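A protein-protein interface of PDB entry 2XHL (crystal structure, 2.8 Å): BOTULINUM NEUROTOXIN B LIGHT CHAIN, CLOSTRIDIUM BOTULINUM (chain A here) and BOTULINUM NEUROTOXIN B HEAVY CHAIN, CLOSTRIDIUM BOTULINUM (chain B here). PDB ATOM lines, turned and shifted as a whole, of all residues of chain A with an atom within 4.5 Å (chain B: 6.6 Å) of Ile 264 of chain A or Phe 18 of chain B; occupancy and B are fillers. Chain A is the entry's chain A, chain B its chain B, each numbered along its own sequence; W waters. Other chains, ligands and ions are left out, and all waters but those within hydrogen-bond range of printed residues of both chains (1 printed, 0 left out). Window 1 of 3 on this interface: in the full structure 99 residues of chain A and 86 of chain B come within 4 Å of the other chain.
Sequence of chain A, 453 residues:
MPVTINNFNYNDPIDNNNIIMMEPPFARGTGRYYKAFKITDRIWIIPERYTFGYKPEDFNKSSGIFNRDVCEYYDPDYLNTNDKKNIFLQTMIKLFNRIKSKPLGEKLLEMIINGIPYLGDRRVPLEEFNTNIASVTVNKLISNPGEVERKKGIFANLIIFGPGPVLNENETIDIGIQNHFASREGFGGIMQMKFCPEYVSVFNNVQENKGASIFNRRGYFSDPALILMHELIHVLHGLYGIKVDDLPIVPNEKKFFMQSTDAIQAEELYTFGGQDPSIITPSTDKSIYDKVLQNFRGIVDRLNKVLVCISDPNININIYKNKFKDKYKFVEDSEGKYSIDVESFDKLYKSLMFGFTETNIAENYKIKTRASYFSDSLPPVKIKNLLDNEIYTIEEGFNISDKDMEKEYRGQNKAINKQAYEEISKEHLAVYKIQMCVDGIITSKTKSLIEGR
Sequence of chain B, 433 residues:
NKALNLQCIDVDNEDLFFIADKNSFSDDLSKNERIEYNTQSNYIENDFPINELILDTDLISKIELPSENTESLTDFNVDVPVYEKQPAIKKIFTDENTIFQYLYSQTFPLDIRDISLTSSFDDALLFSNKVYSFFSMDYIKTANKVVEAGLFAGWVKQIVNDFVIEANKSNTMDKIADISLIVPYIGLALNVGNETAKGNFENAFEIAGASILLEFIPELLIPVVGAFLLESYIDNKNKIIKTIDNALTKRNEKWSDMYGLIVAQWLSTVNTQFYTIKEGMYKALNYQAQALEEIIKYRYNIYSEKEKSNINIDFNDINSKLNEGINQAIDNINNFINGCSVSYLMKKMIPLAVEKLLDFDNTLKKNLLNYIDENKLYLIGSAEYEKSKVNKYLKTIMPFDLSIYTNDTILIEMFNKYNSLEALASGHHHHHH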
ATOM      1  N   PRO A 248      10.684   0.056  -3.711  1.00  0.00           N
ATOM      2  CA  PRO A 248      11.865   0.845  -4.037  1.00  0.00           C
ATOM      3  C   PRO A 248      13.142   0.015  -4.106  1.00  0.00           C
ATOM      4  O   PRO A 248      13.172  -1.117  -3.621  1.00  0.00           O
ATOM      5  CB  PRO A 248      11.949   1.821  -2.862  1.00  0.00           C
ATOM      6  CG  PRO A 248      11.411   1.050  -1.714  1.00  0.00           C
ATOM      7  CD  PRO A 248      10.389   0.085  -2.267  1.00  0.00           C
ATOM      8  N   ILE A 249      14.186   0.576  -4.708  1.00  0.00           N
ATOM      9  CA  ILE A 249      15.517   0.000  -4.594  1.00  0.00           C
ATOM     10  C   ILE A 249      16.087   0.430  -3.248  1.00  0.00           C
ATOM     11  O   ILE A 249      16.242   1.623  -2.975  1.00  0.00           O
ATOM     12  CB  ILE A 249      16.470   0.437  -5.748  1.00  0.00           C
ATOM     13  CG1 ILE A 249      15.912   0.043  -7.126  1.00  0.00           C
ATOM     14  CG2 ILE A 249      17.878  -0.118  -5.529  1.00  0.00           C
ATOM     15  CD1 ILE A 249      15.653  -1.449  -7.335  1.00  0.00           C
ATOM     16  N   PRO A 251      19.383  -0.150  -0.621  1.00  0.00           N
ATOM     17  CA  PRO A 251      20.746  -0.667  -0.559  1.00  0.00           C
ATOM     18  C   PRO A 251      20.945  -1.665   0.580  1.00  0.00           C
ATOM     19  O   PRO A 251      20.351  -1.521   1.653  1.00  0.00           O
ATOM     20  CB  PRO A 251      21.578   0.590  -0.304  1.00  0.00           C
ATOM     21  CG  PRO A 251      20.653   1.492   0.416  1.00  0.00           C
ATOM     22  CD  PRO A 251      19.317   1.264  -0.209  1.00  0.00           C
ATOM     23  N   GLN A 259      27.582   0.981   0.565  1.00  0.00           N
ATOM     24  CA  GLN A 259      27.136   2.370   0.623  1.00  0.00           C
ATOM     25  C   GLN A 259      25.758   2.512   1.276  1.00  0.00           C
ATOM     26  O   GLN A 259      24.851   1.731   0.997  1.00  0.00           O
ATOM     27  CB  GLN A 259      27.121   2.955  -0.790  1.00  0.00           C
ATOM     28  CG  GLN A 259      26.810   4.442  -0.873  1.00  0.00           C
ATOM     29  CD  GLN A 259      27.004   5.012  -2.269  1.00  0.00           C
ATOM     30  OE1 GLN A 259      27.730   4.452  -3.095  1.00  0.00           O
ATOM     31  NE2 GLN A 259      26.358   6.141  -2.537  1.00  0.00           N
ATOM     32  N   THR A 261      22.336   4.689   1.779  1.00  0.00           N
ATOM     33  CA  THR A 261      21.482   5.680   1.131  1.00  0.00           C
ATOM     34  C   THR A 261      20.015   5.412   1.428  1.00  0.00           C
ATOM     35  O   THR A 261      19.656   4.331   1.891  1.00  0.00           O
ATOM     36  CB  THR A 261      21.729   5.768  -0.414  1.00  0.00           C
ATOM     37  OG1 THR A 261      20.795   6.684  -1.008  1.00  0.00           O
ATOM     38  CG2 THR A 261      21.603   4.409  -1.088  1.00  0.00           C
ATOM     39  N   ASP A 262      19.178   6.411   1.166  1.00  0.00           N
ATOM     40  CA  ASP A 262      17.732   6.268   1.287  1.00  0.00           C
ATOM     41  C   ASP A 262      17.181   5.365   0.184  1.00  0.00           C
ATOM     42  O   ASP A 262      17.860   5.096  -0.812  1.00  0.00           O
ATOM     43  CB  ASP A 262      17.053   7.643   1.228  1.00  0.00           C
ATOM     44  CG  ASP A 262      17.465   8.558   2.379  1.00  0.00           C
ATOM     45  OD1 ASP A 262      17.940   8.054   3.427  1.00  0.00           O
ATOM     46  OD2 ASP A 262      17.304   9.794   2.232  1.00  0.00           O
ATOM     47  N   ALA A 263      15.951   4.897   0.378  1.00  0.00           N
ATOM     48  CA  ALA A 263      15.243   4.123  -0.636  1.00  0.00           C
ATOM     49  C   ALA A 263      15.107   4.935  -1.919  1.00  0.00           C
ATOM     50  O   ALA A 263      14.816   6.134  -1.878  1.00  0.00           O
ATOM     51  CB  ALA A 263      13.877   3.710  -0.123  1.00  0.00           C
ATOM     52  N   ILE A 264      15.338   4.277  -3.051  1.00  0.00           N
ATOM     53  CA  ILE A 264      15.245   4.917  -4.358  1.00  0.00           C
ATOM     54  C   ILE A 264      13.995   4.425  -5.090  1.00  0.00           C
ATOM     55  O   ILE A 264      13.880   3.243  -5.430  1.00  0.00           O
ATOM     56  CB  ILE A 264      16.521   4.670  -5.200  1.00  0.00           C
ATOM     57  CG1 ILE A 264      17.766   5.089  -4.407  1.00  0.00           C
ATOM     58  CG2 ILE A 264      16.450   5.424  -6.523  1.00  0.00           C
ATOM     59  CD1 ILE A 264      18.978   4.203  -4.625  1.00  0.00           C
ATOM     60  N   GLN A 265      13.056   5.340  -5.315  1.00  0.00           N
ATOM     61  CA  GLN A 265      11.814   5.014  -6.001  1.00  0.00           C
ATOM     62  C   GLN A 265      11.999   4.942  -7.511  1.00  0.00           C
ATOM     63  O   GLN A 265      12.804   5.678  -8.080  1.00  0.00           O
ATOM     64  CB  GLN A 265      10.723   6.029  -5.658  1.00  0.00           C
ATOM     65  CG  GLN A 265       9.984   5.735  -4.368  1.00  0.00           C
ATOM     66  CD  GLN A 265       9.162   4.456  -4.425  1.00  0.00           C
ATOM     67  OE1 GLN A 265       8.577   4.112  -5.456  1.00  0.00           O
ATOM     68  NE2 GLN A 265       9.112   3.748  -3.307  1.00  0.00           N
ATOM     69  N   ALA A 266      11.237   4.055  -8.146  1.00  0.00           N
ATOM     70  CA  ALA A 266      11.208   3.915  -9.599  1.00  0.00           C
ATOM     71  C   ALA A 266      11.023   5.256 -10.309  1.00  0.00           C
ATOM     72  O   ALA A 266      11.686   5.537 -11.313  1.00  0.00           O
ATOM     73  CB  ALA A 266      10.106   2.957 -10.001  1.00  0.00           C
ATOM     74  N   LEU A 269      14.078   6.936 -11.049  1.00  0.00           N
ATOM     75  CA  LEU A 269      14.852   6.267 -12.097  1.00  0.00           C
ATOM     76  C   LEU A 269      14.234   6.418 -13.489  1.00  0.00           C
ATOM     77  O   LEU A 269      14.957   6.461 -14.486  1.00  0.00           O
ATOM     78  CB  LEU A 269      15.086   4.791 -11.755  1.00  0.00           C
ATOM     79  CG  LEU A 269      16.014   4.491 -10.572  1.00  0.00           C
ATOM     80  CD1 LEU A 269      16.076   2.997 -10.327  1.00  0.00           C
ATOM     81  CD2 LEU A 269      17.421   5.055 -10.774  1.00  0.00           C
ATOM     82  N   TYR A 373      22.335   7.277 -12.692  1.00  0.00           N
ATOM     83  CA  TYR A 373      21.952   7.855 -11.403  1.00  0.00           C
ATOM     84  C   TYR A 373      22.948   7.439 -10.311  1.00  0.00           C
ATOM     85  O   TYR A 373      23.167   8.174  -9.340  1.00  0.00           O
ATOM     86  CB  TYR A 373      20.519   7.436 -11.032  1.00  0.00           C
ATOM     87  CG  TYR A 373      20.093   7.785  -9.623  1.00  0.00           C
ATOM     88  CD1 TYR A 373      19.451   8.991  -9.346  1.00  0.00           C
ATOM     89  CD2 TYR A 373      20.323   6.904  -8.568  1.00  0.00           C
ATOM     90  CE1 TYR A 373      19.057   9.313  -8.046  1.00  0.00           C
ATOM     91  CE2 TYR A 373      19.939   7.216  -7.268  1.00  0.00           C
ATOM     92  CZ  TYR A 373      19.304   8.418  -7.013  1.00  0.00           C
ATOM     93  OH  TYR A 373      18.924   8.721  -5.723  1.00  0.00           O
ATOM     94  N   PHE A 374      23.557   6.269 -10.491  1.00  0.00           N
ATOM     95  CA  PHE A 374      24.464   5.707  -9.499  1.00  0.00           C
ATOM     96  C   PHE A 374      25.927   6.055  -9.750  1.00  0.00           C
ATOM     97  O   PHE A 374      26.825   5.472  -9.134  1.00  0.00           O
ATOM     98  CB  PHE A 374      24.261   4.194  -9.401  1.00  0.00           C
ATOM     99  CG  PHE A 374      22.893   3.808  -8.920  1.00  0.00           C
ATOM    100  CD1 PHE A 374      21.884   3.500  -9.824  1.00  0.00           C
ATOM    101  CD2 PHE A 374      22.607   3.778  -7.560  1.00  0.00           C
ATOM    102  CE1 PHE A 374      20.613   3.155  -9.376  1.00  0.00           C
ATOM    103  CE2 PHE A 374      21.345   3.432  -7.109  1.00  0.00           C
ATOM    104  CZ  PHE A 374      20.346   3.121  -8.015  1.00  0.00           C
ATOM    105  N   LEU B  16      32.179   3.810  -1.691  1.00  0.00           N
ATOM    106  CA  LEU B  16      31.888   2.424  -1.314  1.00  0.00           C
ATOM    107  C   LEU B  16      31.114   1.721  -2.432  1.00  0.00           C
ATOM    108  O   LEU B  16      30.831   2.320  -3.470  1.00  0.00           O
ATOM    109  CB  LEU B  16      31.092   2.361  -0.004  1.00  0.00           C
ATOM    110  CG  LEU B  16      31.520   3.127   1.253  1.00  0.00           C
ATOM    111  CD1 LEU B  16      30.562   2.823   2.397  1.00  0.00           C
ATOM    112  CD2 LEU B  16      32.939   2.806   1.663  1.00  0.00           C
ATOM    113  N   PHE B  17      30.779   0.450  -2.212  1.00  0.00           N
ATOM    114  CA  PHE B  17      30.023  -0.338  -3.186  1.00  0.00           C
ATOM    115  C   PHE B  17      28.531  -0.170  -2.965  1.00  0.00           C
ATOM    116  O   PHE B  17      28.044  -0.381  -1.855  1.00  0.00           O
ATOM    117  CB  PHE B  17      30.357  -1.828  -3.061  1.00  0.00           C
ATOM    118  CG  PHE B  17      31.778  -2.167  -3.390  1.00  0.00           C
ATOM    119  CD1 PHE B  17      32.753  -2.161  -2.399  1.00  0.00           C
ATOM    120  CD2 PHE B  17      32.139  -2.511  -4.687  1.00  0.00           C
ATOM    121  CE1 PHE B  17      34.067  -2.482  -2.698  1.00  0.00           C
ATOM    122  CE2 PHE B  17      33.452  -2.832  -4.997  1.00  0.00           C
ATOM    123  CZ  PHE B  17      34.420  -2.816  -4.002  1.00  0.00           C
ATOM    124  N   PHE B  18      27.806   0.211  -4.014  1.00  0.00           N
ATOM    125  CA  PHE B  18      26.354   0.118  -3.973  1.00  0.00           C
ATOM    126  C   PHE B  18      25.951  -1.284  -4.399  1.00  0.00           C
ATOM    127  O   PHE B  18      26.309  -1.740  -5.487  1.00  0.00           O
ATOM    128  CB  PHE B  18      25.672   1.156  -4.871  1.00  0.00           C
ATOM    129  CG  PHE B  18      24.169   1.179  -4.731  1.00  0.00           C
ATOM    130  CD1 PHE B  18      23.548   2.128  -3.932  1.00  0.00           C
ATOM    131  CD2 PHE B  18      23.378   0.234  -5.382  1.00  0.00           C
ATOM    132  CE1 PHE B  18      22.164   2.143  -3.792  1.00  0.00           C
ATOM    133  CE2 PHE B  18      21.996   0.242  -5.245  1.00  0.00           C
ATOM    134  CZ  PHE B  18      21.389   1.197  -4.448  1.00  0.00           C
ATOM    135  N   ILE B  19      25.219  -1.964  -3.524  1.00  0.00           N
ATOM    136  CA  ILE B  19      24.673  -3.281  -3.814  1.00  0.00           C
ATOM    137  C   ILE B  19      23.213  -3.276  -3.382  1.00  0.00           C
ATOM    138  O   ILE B  19      22.904  -3.049  -2.209  1.00  0.00           O
ATOM    139  CB  ILE B  19      25.452  -4.406  -3.082  1.00  0.00           C
ATOM    140  CG1 ILE B  19      26.906  -4.466  -3.567  1.00  0.00           C
ATOM    141  CG2 ILE B  19      24.768  -5.761  -3.281  1.00  0.00           C
ATOM    142  CD1 ILE B  19      27.868  -5.096  -2.574  1.00  0.00           C
ATOM    143  N   ALA B  20      22.318  -3.510  -4.336  1.00  0.00           N
ATOM    144  CA  ALA B  20      20.888  -3.546  -4.053  1.00  0.00           C
ATOM    145  C   ALA B  20      20.531  -4.757  -3.199  1.00  0.00           C
ATOM    146  O   ALA B  20      21.057  -5.851  -3.405  1.00  0.00           O
ATOM    147  CB  ALA B  20      20.093  -3.549  -5.340  1.00  0.00           C
ATOM    148  N   ASP B  21      19.640  -4.544  -2.237  1.00  0.00           N
ATOM    149  CA  ASP B  21      19.172  -5.602  -1.347  1.00  0.00           C
ATOM    150  C   ASP B  21      18.216  -6.551  -2.072  1.00  0.00           C
ATOM    151  O   ASP B  21      17.644  -6.203  -3.104  1.00  0.00           O
ATOM    152  CB  ASP B  21      18.492  -4.989  -0.117  1.00  0.00           C
ATOM    153  CG  ASP B  21      18.399  -5.959   1.047  1.00  0.00           C
ATOM    154  OD1 ASP B  21      17.515  -6.846   1.028  1.00  0.00           O
ATOM    155  OD2 ASP B  21      19.208  -5.828   1.992  1.00  0.00           O
ATOM    156  N   LEU B 267      22.531  -5.070 -12.984  1.00  0.00           N
ATOM    157  CA  LEU B 267      22.918  -3.663 -13.013  1.00  0.00           C
ATOM    158  C   LEU B 267      23.083  -3.072 -11.616  1.00  0.00           C
ATOM    159  O   LEU B 267      24.063  -2.380 -11.340  1.00  0.00           O
ATOM    160  CB  LEU B 267      21.899  -2.842 -13.804  1.00  0.00           C
ATOM    161  CG  LEU B 267      21.843  -2.982 -15.332  1.00  0.00           C
ATOM    162  CD1 LEU B 267      20.660  -2.213 -15.879  1.00  0.00           C
ATOM    163  CD2 LEU B 267      23.128  -2.504 -16.000  1.00  0.00           C
ATOM    164  N   SER B 268      22.129  -3.360 -10.735  1.00  0.00           N
ATOM    165  CA  SER B 268      22.097  -2.762  -9.404  1.00  0.00           C
ATOM    166  C   SER B 268      22.884  -3.550  -8.352  1.00  0.00           C
ATOM    167  O   SER B 268      22.854  -3.209  -7.169  1.00  0.00           O
ATOM    168  CB  SER B 268      20.648  -2.631  -8.952  1.00  0.00           C
ATOM    169  OG  SER B 268      20.068  -3.917  -8.814  1.00  0.00           O
ATOM    170  N   THR B 269      23.600  -4.584  -8.779  1.00  0.00           N
ATOM    171  CA  THR B 269      24.194  -5.531  -7.839  1.00  0.00           C
ATOM    172  C   THR B 269      25.606  -5.974  -8.231  1.00  0.00           C
ATOM    173  O   THR B 269      26.487  -6.103  -7.371  1.00  0.00           O
ATOM    174  CB  THR B 269      23.258  -6.750  -7.662  1.00  0.00           C
ATOM    175  OG1 THR B 269      22.129  -6.367  -6.860  1.00  0.00           O
ATOM    176  CG2 THR B 269      23.953  -7.894  -7.000  1.00  0.00           C
ATOM    177  N   VAL B 270      25.817  -6.209  -9.522  1.00  0.00           N
ATOM    178  CA  VAL B 270      27.112  -6.669 -10.009  1.00  0.00           C
ATOM    179  C   VAL B 270      27.805  -5.560 -10.792  1.00  0.00           C
ATOM    180  O   VAL B 270      28.969  -5.244 -10.538  1.00  0.00           O
ATOM    181  CB  VAL B 270      26.975  -7.963 -10.856  1.00  0.00           C
ATOM    182  CG1 VAL B 270      28.304  -8.350 -11.499  1.00  0.00           C
ATOM    183  CG2 VAL B 270      26.461  -9.105  -9.993  1.00  0.00           C
ATOM    184  N   THR B 272      27.430  -2.398 -10.687  1.00  0.00           N
ATOM    185  CA  THR B 272      27.816  -1.283  -9.824  1.00  0.00           C
ATOM    186  C   THR B 272      29.164  -1.532  -9.153  1.00  0.00           C
ATOM    187  O   THR B 272      29.958  -0.604  -8.994  1.00  0.00           O
ATOM    188  CB  THR B 272      26.762  -0.982  -8.739  1.00  0.00           C
ATOM    189  OG1 THR B 272      26.291  -2.209  -8.163  1.00  0.00           O
ATOM    190  CG2 THR B 272      25.599  -0.219  -9.327  1.00  0.00           C
ATOM    191  N   GLN B 273      29.416  -2.781  -8.762  1.00  0.00           N
ATOM    192  CA  GLN B 273      30.693  -3.161  -8.162  1.00  0.00           C
ATOM    193  C   GLN B 273      31.833  -2.943  -9.141  1.00  0.00           C
ATOM    194  O   GLN B 273      32.864  -2.384  -8.785  1.00  0.00           O
ATOM    195  CB  GLN B 273      30.682  -4.621  -7.703  1.00  0.00           C
ATOM    196  CG  GLN B 273      29.741  -4.909  -6.551  1.00  0.00           C
ATOM    197  CD  GLN B 273      29.914  -6.307  -6.003  1.00  0.00           C
ATOM    198  OE1 GLN B 273      30.978  -6.657  -5.493  1.00  0.00           O
ATOM    199  NE2 GLN B 273      28.864  -7.114  -6.100  1.00  0.00           N
ATOM    200  N   THR B 276      32.791   0.691  -9.467  1.00  0.00           N
ATOM    201  CA  THR B 276      33.659   1.101  -8.369  1.00  0.00           C
ATOM    202  C   THR B 276      35.099   0.669  -8.645  1.00  0.00           C
ATOM    203  O   THR B 276      36.032   1.452  -8.461  1.00  0.00           O
ATOM    204  CB  THR B 276      33.176   0.510  -7.022  1.00  0.00           C
ATOM    205  OG1 THR B 276      31.785   0.795  -6.847  1.00  0.00           O
ATOM    206  CG2 THR B 276      33.950   1.104  -5.853  1.00  0.00           C
HETATM  207  O   HOH W   1      24.656  -0.849  -0.614  1.00  0.00           O
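N of Gln 259 of chain A is in hydrogen-bond range of O of Phe 17 of chain B, 2.8 Å away.
The backbone NH (N) of Ile 249 of chain A lies within hydrogen-bond range of the backbone carbonyl oxygen (O) of Ile 264 of chain A, 2.8 Å away.
The backbone carbonyl oxygen (O) of Phe 18 of chain B lies within hydrogen-bond range of the side-chain hydroxyl (OG1) of Thr 272 of chain B.
Phe 18 of chain B touches Ile 249 of chain A.
Pro 251 of chain A touches Phe 18 of chain B (CB to CE1, 3.9 Å).
Ile 19 of chain B touches Pro 251 of chain A.
Gln 259 of chain A touches Leu 16 of chain B.
Thr 261 of chain A touches Phe 18 of chain B (CG2 to CE1, 3.6 Å).
CD1 of Ile 264 of chain A touches CZ of Phe 18 of chain B, at 3.9 Å.
CZ of Phe 18 of chain B touches CE2 of Phe 374 of chain A, at 3.5 Å.
Ile 264 of chain A touches just one residue of chain B: Phe 18.
Printed residues of chain A within 4 Å of Leu 16 of chain B: Gln 259 (3.8 Å).
Printed residues of chain A within 4 Å of Phe 17 of chain B: Gln 259 (2.8 Å).
Of the printed residues of chain B, Phe 374 of chain A touches Phe 18 (3.5 Å).
Val 270 of chain B touches none of the printed residues of chain A.
The nearest printed residue of chain B that does not touch Ile 264 of chain A is Ala 20 of chain B (7.9 Å).
The nearest residue of chain A that does not touch Phe 18 of chain B is Gln 259 of chain A (4.3 Å).
The nearest printed residue of chain B that does not touch Phe 374 of chain A is Thr 272 of chain B (4.6 Å).
Of the 13 printed residues of chain A, 6 touch a printed residue of chain B.
Printed residues of chain A that touch a printed residue of chain B: Ile 249, Pro 251, Gln 259, Thr 261, Ile 264 and Phe 374.
Printed residues of chain B that touch a printed residue of chain A: Leu 16, Phe 17, Phe 18 and Ile 19.
Hydrophobic or aromatic side chains of chain B within 4 Å of the printed part of chain A: Leu 16 and Phe 18.
Among the printed residues, 8 pairs touch across the chains.
Water W1 bridges O of Gln 259 of chain A (3.0 Å) and N of Ile 19 of chain B (3.2 Å).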
